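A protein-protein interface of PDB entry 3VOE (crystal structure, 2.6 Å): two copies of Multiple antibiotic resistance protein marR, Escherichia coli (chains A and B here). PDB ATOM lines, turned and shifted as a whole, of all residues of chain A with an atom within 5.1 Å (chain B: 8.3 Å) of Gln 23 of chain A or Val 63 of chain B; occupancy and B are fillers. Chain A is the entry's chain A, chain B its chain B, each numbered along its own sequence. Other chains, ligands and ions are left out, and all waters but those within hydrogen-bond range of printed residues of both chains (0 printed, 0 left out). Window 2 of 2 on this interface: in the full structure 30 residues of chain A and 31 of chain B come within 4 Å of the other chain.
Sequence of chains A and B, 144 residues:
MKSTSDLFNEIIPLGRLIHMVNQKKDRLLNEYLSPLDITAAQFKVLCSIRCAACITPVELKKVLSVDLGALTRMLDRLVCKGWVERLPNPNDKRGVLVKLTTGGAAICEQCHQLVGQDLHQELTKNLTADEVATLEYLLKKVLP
ND2 of Asn 22 of chain B sits close to ND2 of Asn 22 of chain A (3.1 Å). The side-chain amide oxygen (OE1) of Gln 23 of chain A lies close to the backbone carbonyl oxygen (O) of Val 63 of chain B, 3.1 Å away. NZ of Lys 24 of chain A is in hydrogen-bond range of O of Leu 143 of chain B (3.4 Å).
The side-chain hydroxyl of Ser 48 of chain B lies within hydrogen-bond range of the backbone carbonyl oxygen of Lys 44 of chain B, at 2.8 Å.
Asn 22 of chain B touches Ile 18 of chain A (CA to CG2, 3.6 Å). Asn 22 of chain B touches His 19 of chain A (OD1 to CA, 3.9 Å). His 19 of chain A touches Lys 44 of chain B. Met 20 of chain A touches Leu 143 of chain B (CE to CD1, 3.7 Å). Val 21 of chain A touches Ile 18 of chain B (CG1 to CD1, 3.4 Å). CG2 of Val 21 of chain A touches CD2 of Leu 143 of chain B, 3.7 Å away. Ile 18 of chain B touches Asn 22 of chain A (CG2 to CA, 3.6 Å).
Of chain B, only Val 63 (3.1 Å) comes within 4 Å of Gln 23 of chain A. Val 63 of chain B touches one residue of chain A. Of the printed residues of chain B, Val 21 of chain A touches Ile 18 (3.4 Å) and Leu 143 (3.7 Å). Printed residues of chain B within 4 Å of Ile 18 of chain A: Asn 22 (3.6 Å). Printed residues of chain A within 4 Å of Ile 18 of chain B: Val 21 (3.4 Å) and Asn 22 (3.6 Å). Lys 61 of chain B touches none of the printed residues of chain A. Cys 47 of chain B touches none of the printed residues of chain A. The nearest residue of chain B that does not touch Gln 23 of chain A is Ser 65 of chain B (4.7 Å). The nearest printed residue of chain A that does not touch Val 63 of chain B is His 19 of chain A (5.8 Å).
Of the 23 printed residues of chain B, 5 touch a printed residue of chain A. Hydrophobic or aromatic side chains of chain B within 4 Å of the printed part of chain A: Ile 18 and Leu 143. Hydrophobic or aromatic side chains of chain A within 4 Å of the printed part of chain B: Ile 18, His 19, Met 20 and Val 21. Among the printed residues, no Asp or Glu carboxylate lies within 4 Å of a Lys or Arg side-chain nitrogen of the other chain.
Ile 18 of chain A touches Asn 22 of chain B, and with the chains exchanged Asn 22 of chain A touches Ile 18 of chain B. Asn 22 of chain B touches its own counterpart, Asn 22 of chain A. 2 positions are printed for both chains.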
ATOM      1  N   ILE A  18     -16.745  -6.225  17.542  1.00  0.00           N
ATOM      2  CA  ILE A  18     -16.205  -6.543  16.234  1.00  0.00           C
ATOM      3  C   ILE A  18     -15.565  -5.319  15.584  1.00  0.00           C
ATOM      4  O   ILE A  18     -14.511  -5.426  14.962  1.00  0.00           O
ATOM      5  CB  ILE A  18     -17.273  -7.149  15.306  1.00  0.00           C
ATOM      6  CG1 ILE A  18     -17.437  -8.637  15.602  1.00  0.00           C
ATOM      7  CG2 ILE A  18     -16.897  -6.951  13.844  1.00  0.00           C
ATOM      8  CD1 ILE A  18     -18.875  -9.090  15.618  1.00  0.00           C
ATOM      9  N   HIS A  19     -16.176  -4.149  15.772  1.00  0.00           N
ATOM     10  CA  HIS A  19     -15.606  -2.909  15.248  1.00  0.00           C
ATOM     11  C   HIS A  19     -14.239  -2.614  15.835  1.00  0.00           C
ATOM     12  O   HIS A  19     -13.264  -2.417  15.100  1.00  0.00           O
ATOM     13  CB  HIS A  19     -16.545  -1.736  15.473  1.00  0.00           C
ATOM     14  CG  HIS A  19     -16.245  -0.546  14.598  1.00  0.00           C
ATOM     15  ND1 HIS A  19     -15.520   0.509  15.026  1.00  0.00           N
ATOM     16  CD2 HIS A  19     -16.555  -0.289  13.258  1.00  0.00           C
ATOM     17  CE1 HIS A  19     -15.392   1.398  14.026  1.00  0.00           C
ATOM     18  NE2 HIS A  19     -16.024   0.911  12.947  1.00  0.00           N
ATOM     19  N   MET A  20     -14.159  -2.601  17.164  1.00  0.00           N
ATOM     20  CA  MET A  20     -12.906  -2.317  17.864  1.00  0.00           C
ATOM     21  C   MET A  20     -11.795  -3.290  17.467  1.00  0.00           C
ATOM     22  O   MET A  20     -10.661  -2.876  17.183  1.00  0.00           O
ATOM     23  CB  MET A  20     -13.122  -2.354  19.373  1.00  0.00           C
ATOM     24  CG  MET A  20     -14.040  -1.259  19.893  1.00  0.00           C
ATOM     25  SD  MET A  20     -14.585  -1.543  21.588  1.00  0.00           S
ATOM     26  CE  MET A  20     -13.037  -1.373  22.477  1.00  0.00           C
ATOM     27  N   VAL A  21     -12.128  -4.578  17.437  1.00  0.00           N
ATOM     28  CA  VAL A  21     -11.166  -5.621  17.062  1.00  0.00           C
ATOM     29  C   VAL A  21     -10.774  -5.534  15.577  1.00  0.00           C
ATOM     30  O   VAL A  21      -9.629  -5.818  15.208  1.00  0.00           O
ATOM     31  CB  VAL A  21     -11.703  -7.033  17.395  1.00  0.00           C
ATOM     32  CG1 VAL A  21     -10.728  -8.104  16.929  1.00  0.00           C
ATOM     33  CG2 VAL A  21     -11.952  -7.159  18.891  1.00  0.00           C
ATOM     34  N   ASN A  22     -11.721  -5.120  14.738  1.00  0.00           N
ATOM     35  CA  ASN A  22     -11.424  -4.838  13.338  1.00  0.00           C
ATOM     36  C   ASN A  22     -10.483  -3.648  13.185  1.00  0.00           C
ATOM     37  O   ASN A  22      -9.479  -3.724  12.473  1.00  0.00           O
ATOM     38  CB  ASN A  22     -12.705  -4.595  12.551  1.00  0.00           C
ATOM     39  CG  ASN A  22     -12.453  -4.446  11.067  1.00  0.00           C
ATOM     40  OD1 ASN A  22     -12.074  -5.404  10.390  1.00  0.00           O
ATOM     41  ND2 ASN A  22     -12.653  -3.239  10.553  1.00  0.00           N
ATOM     42  N   GLN A  23     -10.804  -2.555  13.870  1.00  0.00           N
ATOM     43  CA  GLN A  23      -9.992  -1.352  13.811  1.00  0.00           C
ATOM     44  C   GLN A  23      -8.561  -1.615  14.286  1.00  0.00           C
ATOM     45  O   GLN A  23      -7.604  -1.137  13.677  1.00  0.00           O
ATOM     46  CB  GLN A  23     -10.629  -0.232  14.627  1.00  0.00           C
ATOM     47  CG  GLN A  23     -10.287   1.158  14.126  1.00  0.00           C
ATOM     48  CD  GLN A  23     -10.799   2.248  15.040  1.00  0.00           C
ATOM     49  OE1 GLN A  23     -11.996   2.544  15.065  1.00  0.00           O
ATOM     50  NE2 GLN A  23      -9.893   2.863  15.796  1.00  0.00           N
ATOM     51  N   LYS A  24      -8.422  -2.391  15.366  1.00  0.00           N
ATOM     52  CA  LYS A  24      -7.104  -2.833  15.830  1.00  0.00           C
ATOM     53  C   LYS A  24      -6.373  -3.626  14.747  1.00  0.00           C
ATOM     54  O   LYS A  24      -5.181  -3.399  14.496  1.00  0.00           O
ATOM     55  CB  LYS A  24      -7.224  -3.669  17.111  1.00  0.00           C
ATOM     56  CG  LYS A  24      -5.959  -4.453  17.455  1.00  0.00           C
ATOM     57  CD  LYS A  24      -5.983  -4.995  18.872  1.00  0.00           C
ATOM     58  CE  LYS A  24      -4.749  -5.844  19.142  1.00  0.00           C
ATOM     59  NZ  LYS A  24      -4.248  -5.690  20.537  1.00  0.00           N
ATOM     60  N   LYS A  25      -7.091  -4.550  14.107  1.00  0.00           N
ATOM     61  CA  LYS A  25      -6.538  -5.329  12.998  1.00  0.00           C
ATOM     62  C   LYS A  25      -6.017  -4.418  11.889  1.00  0.00           C
ATOM     63  O   LYS A  25      -4.926  -4.632  11.358  1.00  0.00           O
ATOM     64  CB  LYS A  25      -7.592  -6.295  12.436  1.00  0.00           C
ATOM     65  CG  LYS A  25      -7.140  -7.062  11.199  1.00  0.00           C
ATOM     66  CD  LYS A  25      -8.326  -7.637  10.442  1.00  0.00           C
ATOM     67  CE  LYS A  25      -9.062  -6.566   9.651  1.00  0.00           C
ATOM     68  NZ  LYS A  25      -8.351  -6.213   8.394  1.00  0.00           N
ATOM     69  N   ASP A  26      -6.802  -3.400  11.548  1.00  0.00           N
ATOM     70  CA  ASP A  26      -6.426  -2.467  10.491  1.00  0.00           C
ATOM     71  C   ASP A  26      -5.156  -1.697  10.834  1.00  0.00           C
ATOM     72  O   ASP A  26      -4.313  -1.465   9.968  1.00  0.00           O
ATOM     73  CB  ASP A  26      -7.576  -1.499  10.184  1.00  0.00           C
ATOM     74  CG  ASP A  26      -8.535  -2.042   9.134  1.00  0.00           C
ATOM     75  OD1 ASP A  26      -8.107  -2.871   8.297  1.00  0.00           O
ATOM     76  OD2 ASP A  26      -9.717  -1.638   9.141  1.00  0.00           O
ATOM     77  N   ARG A  27      -5.025  -1.306  12.103  1.00  0.00           N
ATOM     78  CA  ARG A  27      -3.857  -0.545  12.564  1.00  0.00           C
ATOM     79  C   ARG A  27      -2.590  -1.395  12.551  1.00  0.00           C
ATOM     80  O   ARG A  27      -1.538  -0.947  12.092  1.00  0.00           O
ATOM     81  CB  ARG A  27      -4.094   0.023  13.968  1.00  0.00           C
ATOM     82  CG  ARG A  27      -5.171   1.100  14.043  1.00  0.00           C
ATOM     83  CD  ARG A  27      -5.153   1.806  15.393  1.00  0.00           C
ATOM     84  NE  ARG A  27      -4.932   0.871  16.499  1.00  0.00           N
ATOM     85  CZ  ARG A  27      -5.862   0.512  17.383  1.00  0.00           C
ATOM     86  NH1 ARG A  27      -7.089   1.019  17.311  1.00  0.00           N
ATOM     87  NH2 ARG A  27      -5.562  -0.351  18.345  1.00  0.00           N
ATOM     88  N   ILE B  18     -12.699 -11.682  11.167  1.00  0.00           N
ATOM     89  CA  ILE B  18     -13.104 -10.409  11.737  1.00  0.00           C
ATOM     90  C   ILE B  18     -13.512  -9.415  10.650  1.00  0.00           C
ATOM     91  O   ILE B  18     -14.492  -8.695  10.806  1.00  0.00           O
ATOM     92  CB  ILE B  18     -12.005  -9.810  12.646  1.00  0.00           C
ATOM     93  CG1 ILE B  18     -12.050 -10.468  14.025  1.00  0.00           C
ATOM     94  CG2 ILE B  18     -12.184  -8.304  12.794  1.00  0.00           C
ATOM     95  CD1 ILE B  18     -10.698 -10.591  14.684  1.00  0.00           C
ATOM     96  N   ASN B  22     -17.225  -8.069  10.324  1.00  0.00           N
ATOM     97  CA  ASN B  22     -17.368  -6.602  10.341  1.00  0.00           C
ATOM     98  C   ASN B  22     -18.213  -6.076   9.178  1.00  0.00           C
ATOM     99  O   ASN B  22     -19.118  -5.265   9.379  1.00  0.00           O
ATOM    100  CB  ASN B  22     -16.000  -5.923  10.341  1.00  0.00           C
ATOM    101  CG  ASN B  22     -16.090  -4.429  10.588  1.00  0.00           C
ATOM    102  OD1 ASN B  22     -16.572  -3.985  11.634  1.00  0.00           O
ATOM    103  ND2 ASN B  22     -15.609  -3.644   9.632  1.00  0.00           N
ATOM    104  N   LYS B  44     -21.231   6.109  11.783  1.00  0.00           N
ATOM    105  CA  LYS B  44     -19.939   5.974  12.437  1.00  0.00           C
ATOM    106  C   LYS B  44     -19.306   7.340  12.690  1.00  0.00           C
ATOM    107  O   LYS B  44     -18.660   7.557  13.726  1.00  0.00           O
ATOM    108  CB  LYS B  44     -19.005   5.114  11.589  1.00  0.00           C
ATOM    109  CG  LYS B  44     -19.380   3.647  11.554  1.00  0.00           C
ATOM    110  CD  LYS B  44     -18.489   2.879  10.597  1.00  0.00           C
ATOM    111  CE  LYS B  44     -18.738   1.387  10.707  1.00  0.00           C
ATOM    112  NZ  LYS B  44     -18.032   0.642   9.634  1.00  0.00           N
ATOM    113  N   VAL B  45     -19.497   8.260  11.743  1.00  0.00           N
ATOM    114  CA  VAL B  45     -18.956   9.613  11.860  1.00  0.00           C
ATOM    115  C   VAL B  45     -19.583  10.347  13.047  1.00  0.00           C
ATOM    116  O   VAL B  45     -18.871  10.875  13.906  1.00  0.00           O
ATOM    117  CB  VAL B  45     -19.174  10.433  10.563  1.00  0.00           C
ATOM    118  CG1 VAL B  45     -18.909  11.914  10.808  1.00  0.00           C
ATOM    119  CG2 VAL B  45     -18.290   9.905   9.443  1.00  0.00           C
ATOM    120  N   CYS B  47     -21.068   9.167  15.656  1.00  0.00           N
ATOM    121  CA  CYS B  47     -20.624   8.515  16.898  1.00  0.00           C
ATOM    122  C   CYS B  47     -19.238   8.959  17.336  1.00  0.00           C
ATOM    123  O   CYS B  47     -19.020   9.271  18.500  1.00  0.00           O
ATOM    124  CB  CYS B  47     -20.651   7.007  16.743  1.00  0.00           C
ATOM    125  SG  CYS B  47     -22.306   6.328  16.674  1.00  0.00           S
ATOM    126  N   SER B  48     -18.295   8.951  16.403  1.00  0.00           N
ATOM    127  CA  SER B  48     -16.933   9.345  16.703  1.00  0.00           C
ATOM    128  C   SER B  48     -16.881  10.785  17.198  1.00  0.00           C
ATOM    129  O   SER B  48     -16.227  11.080  18.200  1.00  0.00           O
ATOM    130  CB  SER B  48     -16.047   9.161  15.481  1.00  0.00           C
ATOM    131  OG  SER B  48     -16.140   7.826  14.992  1.00  0.00           O
ATOM    132  N   ILE B  49     -17.626  11.669  16.524  1.00  0.00           N
ATOM    133  CA  ILE B  49     -17.744  13.077  16.944  1.00  0.00           C
ATOM    134  C   ILE B  49     -18.442  13.211  18.299  1.00  0.00           C
ATOM    135  O   ILE B  49     -18.229  14.190  19.028  1.00  0.00           O
ATOM    136  CB  ILE B  49     -18.527  13.921  15.908  1.00  0.00           C
ATOM    137  CG1 ILE B  49     -17.763  14.005  14.596  1.00  0.00           C
ATOM    138  CG2 ILE B  49     -18.794  15.320  16.441  1.00  0.00           C
ATOM    139  CD1 ILE B  49     -18.394  14.938  13.577  1.00  0.00           C
ATOM    140  N   CYS B  51     -18.231  10.947  20.748  1.00  0.00           N
ATOM    141  CA  CYS B  51     -17.345  10.412  21.792  1.00  0.00           C
ATOM    142  C   CYS B  51     -16.355  11.444  22.297  1.00  0.00           C
ATOM    143  O   CYS B  51     -16.076  11.506  23.492  1.00  0.00           O
ATOM    144  CB  CYS B  51     -16.604   9.181  21.293  1.00  0.00           C
ATOM    145  SG  CYS B  51     -17.648   7.722  21.157  1.00  0.00           S
ATOM    146  N   ALA B  52     -15.782  12.216  21.380  1.00  0.00           N
ATOM    147  CA  ALA B  52     -15.192  13.476  21.769  1.00  0.00           C
ATOM    148  C   ALA B  52     -16.330  14.472  21.937  1.00  0.00           C
ATOM    149  O   ALA B  52     -17.479  14.180  21.557  1.00  0.00           O
ATOM    150  CB  ALA B  52     -14.150  13.973  20.675  1.00  0.00           C
ATOM    151  N   ILE B  55     -13.730  17.541  17.893  1.00  0.00           N
ATOM    152  CA  ILE B  55     -12.656  16.830  17.213  1.00  0.00           C
ATOM    153  C   ILE B  55     -12.369  17.490  15.858  1.00  0.00           C
ATOM    154  O   ILE B  55     -13.245  18.129  15.277  1.00  0.00           O
ATOM    155  CB  ILE B  55     -13.009  15.332  17.023  1.00  0.00           C
ATOM    156  CG1 ILE B  55     -11.779  14.535  16.579  1.00  0.00           C
ATOM    157  CG2 ILE B  55     -14.173  15.166  16.050  1.00  0.00           C
ATOM    158  CD1 ILE B  55     -11.883  13.044  16.843  1.00  0.00           C
ATOM    159  N   THR B  56     -11.131  17.375  15.388  1.00  0.00           N
ATOM    160  CA  THR B  56     -10.763  17.924  14.082  1.00  0.00           C
ATOM    161  C   THR B  56     -10.870  16.852  13.003  1.00  0.00           C
ATOM    162  O   THR B  56     -10.714  15.666  13.291  1.00  0.00           O
ATOM    163  CB  THR B  56      -9.329  18.505  14.085  1.00  0.00           C
ATOM    164  OG1 THR B  56      -8.391  17.478  14.427  1.00  0.00           O
ATOM    165  CG2 THR B  56      -9.213  19.651  15.077  1.00  0.00           C
ATOM    166  N   PRO B  57     -11.145  17.270  11.749  1.00  0.00           N
ATOM    167  CA  PRO B  57     -11.214  16.343  10.615  1.00  0.00           C
ATOM    168  C   PRO B  57      -9.997  15.419  10.545  1.00  0.00           C
ATOM    169  O   PRO B  57     -10.139  14.228  10.268  1.00  0.00           O
ATOM    170  CB  PRO B  57     -11.238  17.279   9.411  1.00  0.00           C
ATOM    171  CG  PRO B  57     -11.922  18.501   9.912  1.00  0.00           C
ATOM    172  CD  PRO B  57     -11.531  18.642  11.361  1.00  0.00           C
ATOM    173  N   VAL B  58      -8.814  15.972  10.805  1.00  0.00           N
ATOM    174  CA  VAL B  58      -7.580  15.195  10.796  1.00  0.00           C
ATOM    175  C   VAL B  58      -7.626  14.113  11.863  1.00  0.00           C
ATOM    176  O   VAL B  58      -7.323  12.948  11.594  1.00  0.00           O
ATOM    177  CB  VAL B  58      -6.348  16.087  11.044  1.00  0.00           C
ATOM    178  CG1 VAL B  58      -5.070  15.318  10.743  1.00  0.00           C
ATOM    179  CG2 VAL B  58      -6.430  17.353  10.204  1.00  0.00           C
ATOM    180  N   GLU B  59      -8.009  14.509  13.077  1.00  0.00           N
ATOM    181  CA  GLU B  59      -8.128  13.580  14.197  1.00  0.00           C
ATOM    182  C   GLU B  59      -9.265  12.599  13.956  1.00  0.00           C
ATOM    183  O   GLU B  59      -9.202  11.444  14.383  1.00  0.00           O
ATOM    184  CB  GLU B  59      -8.363  14.349  15.500  1.00  0.00           C
ATOM    185  CG  GLU B  59      -7.834  13.651  16.746  1.00  0.00           C
ATOM    186  CD  GLU B  59      -6.328  13.807  16.917  1.00  0.00           C
ATOM    187  OE1 GLU B  59      -5.750  14.751  16.332  1.00  0.00           O
ATOM    188  OE2 GLU B  59      -5.722  12.987  17.642  1.00  0.00           O
ATOM    189  N   LEU B  60     -10.298  13.067  13.255  1.00  0.00           N
ATOM    190  CA  LEU B  60     -11.448  12.238  12.907  1.00  0.00           C
ATOM    191  C   LEU B  60     -11.101  11.222  11.817  1.00  0.00           C
ATOM    192  O   LEU B  60     -11.656  10.125  11.784  1.00  0.00           O
ATOM    193  CB  LEU B  60     -12.617  13.121  12.454  1.00  0.00           C
ATOM    194  CG  LEU B  60     -14.016  12.498  12.383  1.00  0.00           C
ATOM    195  CD1 LEU B  60     -14.483  12.041  13.758  1.00  0.00           C
ATOM    196  CD2 LEU B  60     -15.007  13.487  11.784  1.00  0.00           C
ATOM    197  N   LYS B  61     -10.181  11.599  10.928  1.00  0.00           N
ATOM    198  CA  LYS B  61      -9.693  10.686   9.891  1.00  0.00           C
ATOM    199  C   LYS B  61      -8.959   9.493  10.498  1.00  0.00           C
ATOM    200  O   LYS B  61      -9.134   8.359  10.057  1.00  0.00           O
ATOM    201  CB  LYS B  61      -8.775  11.420   8.902  1.00  0.00           C
ATOM    202  CG  LYS B  61      -8.201  10.522   7.812  1.00  0.00           C
ATOM    203  CD  LYS B  61      -6.968  11.127   7.166  1.00  0.00           C
ATOM    204  CE  LYS B  61      -6.306  10.136   6.220  1.00  0.00           C
ATOM    205  NZ  LYS B  61      -5.110  10.719   5.547  1.00  0.00           N
ATOM    206  N   LYS B  62      -8.131   9.760  11.506  1.00  0.00           N
ATOM    207  CA  LYS B  62      -7.321   8.716  12.140  1.00  0.00           C
ATOM    208  C   LYS B  62      -8.198   7.672  12.837  1.00  0.00           C
ATOM    209  O   LYS B  62      -8.063   6.473  12.588  1.00  0.00           O
ATOM    210  CB  LYS B  62      -6.322   9.325  13.139  1.00  0.00           C
ATOM    211  CG  LYS B  62      -5.279  10.249  12.515  1.00  0.00           C
ATOM    212  CD  LYS B  62      -4.050  10.373  13.409  1.00  0.00           C
ATOM    213  CE  LYS B  62      -3.434  11.763  13.328  1.00  0.00           C
ATOM    214  NZ  LYS B  62      -4.098  12.719  14.260  1.00  0.00           N
ATOM    215  N   VAL B  63      -9.110   8.140  13.692  1.00  0.00           N
ATOM    216  CA  VAL B  63     -10.010   7.250  14.438  1.00  0.00           C
ATOM    217  C   VAL B  63     -10.856   6.381  13.499  1.00  0.00           C
ATOM    218  O   VAL B  63     -10.941   5.166  13.676  1.00  0.00           O
ATOM    219  CB  VAL B  63     -10.938   8.044  15.391  1.00  0.00           C
ATOM    220  CG1 VAL B  63     -11.959   7.121  16.040  1.00  0.00           C
ATOM    221  CG2 VAL B  63     -10.120   8.765  16.454  1.00  0.00           C
ATOM    222  N   LEU B  64     -11.458   7.009  12.490  1.00  0.00           N
ATOM    223  CA  LEU B  64     -12.332   6.299  11.548  1.00  0.00           C
ATOM    224  C   LEU B  64     -11.551   5.468  10.526  1.00  0.00           C
ATOM    225  O   LEU B  64     -12.046   4.449  10.045  1.00  0.00           O
ATOM    226  CB  LEU B  64     -13.254   7.279  10.825  1.00  0.00           C
ATOM    227  CG  LEU B  64     -14.433   7.836  11.618  1.00  0.00           C
ATOM    228  CD1 LEU B  64     -14.963   9.096  10.952  1.00  0.00           C
ATOM    229  CD2 LEU B  64     -15.534   6.795  11.759  1.00  0.00           C
ATOM    230  N   SER B  65     -10.342   5.918  10.192  1.00  0.00           N
ATOM    231  CA  SER B  65      -9.498   5.247   9.178  1.00  0.00           C
ATOM    232  C   SER B  65     -10.132   5.267   7.784  1.00  0.00           C
ATOM    233  O   SER B  65     -10.196   4.240   7.103  1.00  0.00           O
ATOM    234  CB  SER B  65      -9.167   3.801   9.598  1.00  0.00           C
ATOM    235  OG  SER B  65      -8.295   3.777  10.711  1.00  0.00           O
ATOM    236  N   VAL B  66     -10.597   6.442   7.370  1.00  0.00           N
ATOM    237  CA  VAL B  66     -11.153   6.622   6.029  1.00  0.00           C
ATOM    238  C   VAL B  66     -10.488   7.787   5.305  1.00  0.00           C
ATOM    239  O   VAL B  66      -9.865   8.643   5.934  1.00  0.00           O
ATOM    240  CB  VAL B  66     -12.685   6.838   6.062  1.00  0.00           C
ATOM    241  CG1 VAL B  66     -13.399   5.540   6.407  1.00  0.00           C
ATOM    242  CG2 VAL B  66     -13.054   7.941   7.049  1.00  0.00           C
ATOM    243  N   LEU B  71     -14.188  12.003   3.521  1.00  0.00           N
ATOM    244  CA  LEU B  71     -14.627  12.420   4.849  1.00  0.00           C
ATOM    245  C   LEU B  71     -15.015  13.905   4.879  1.00  0.00           C
ATOM    246  O   LEU B  71     -15.989  14.289   5.543  1.00  0.00           O
ATOM    247  CB  LEU B  71     -13.538  12.133   5.881  1.00  0.00           C
ATOM    248  CG  LEU B  71     -13.705  12.749   7.264  1.00  0.00           C
ATOM    249  CD1 LEU B  71     -14.931  12.179   7.957  1.00  0.00           C
ATOM    250  CD2 LEU B  71     -12.455  12.519   8.102  1.00  0.00           C
ATOM    251  N   LEU B 143      -8.236  -7.413  22.707  1.00  0.00           N
ATOM    252  CA  LEU B 143      -8.218  -5.940  22.628  1.00  0.00           C
ATOM    253  C   LEU B 143      -7.041  -5.259  23.373  1.00  0.00           C
ATOM    254  O   LEU B 143      -6.356  -4.395  22.799  1.00  0.00           O
ATOM    255  CB  LEU B 143      -9.556  -5.355  23.091  1.00  0.00           C
ATOM    256  CG  LEU B 143     -10.677  -5.361  22.057  1.00  0.00           C
ATOM    257  CD1 LEU B 143     -11.992  -4.934  22.686  1.00  0.00           C
ATOM    258  CD2 LEU B 143     -10.325  -4.467  20.878  1.00  0.00           C
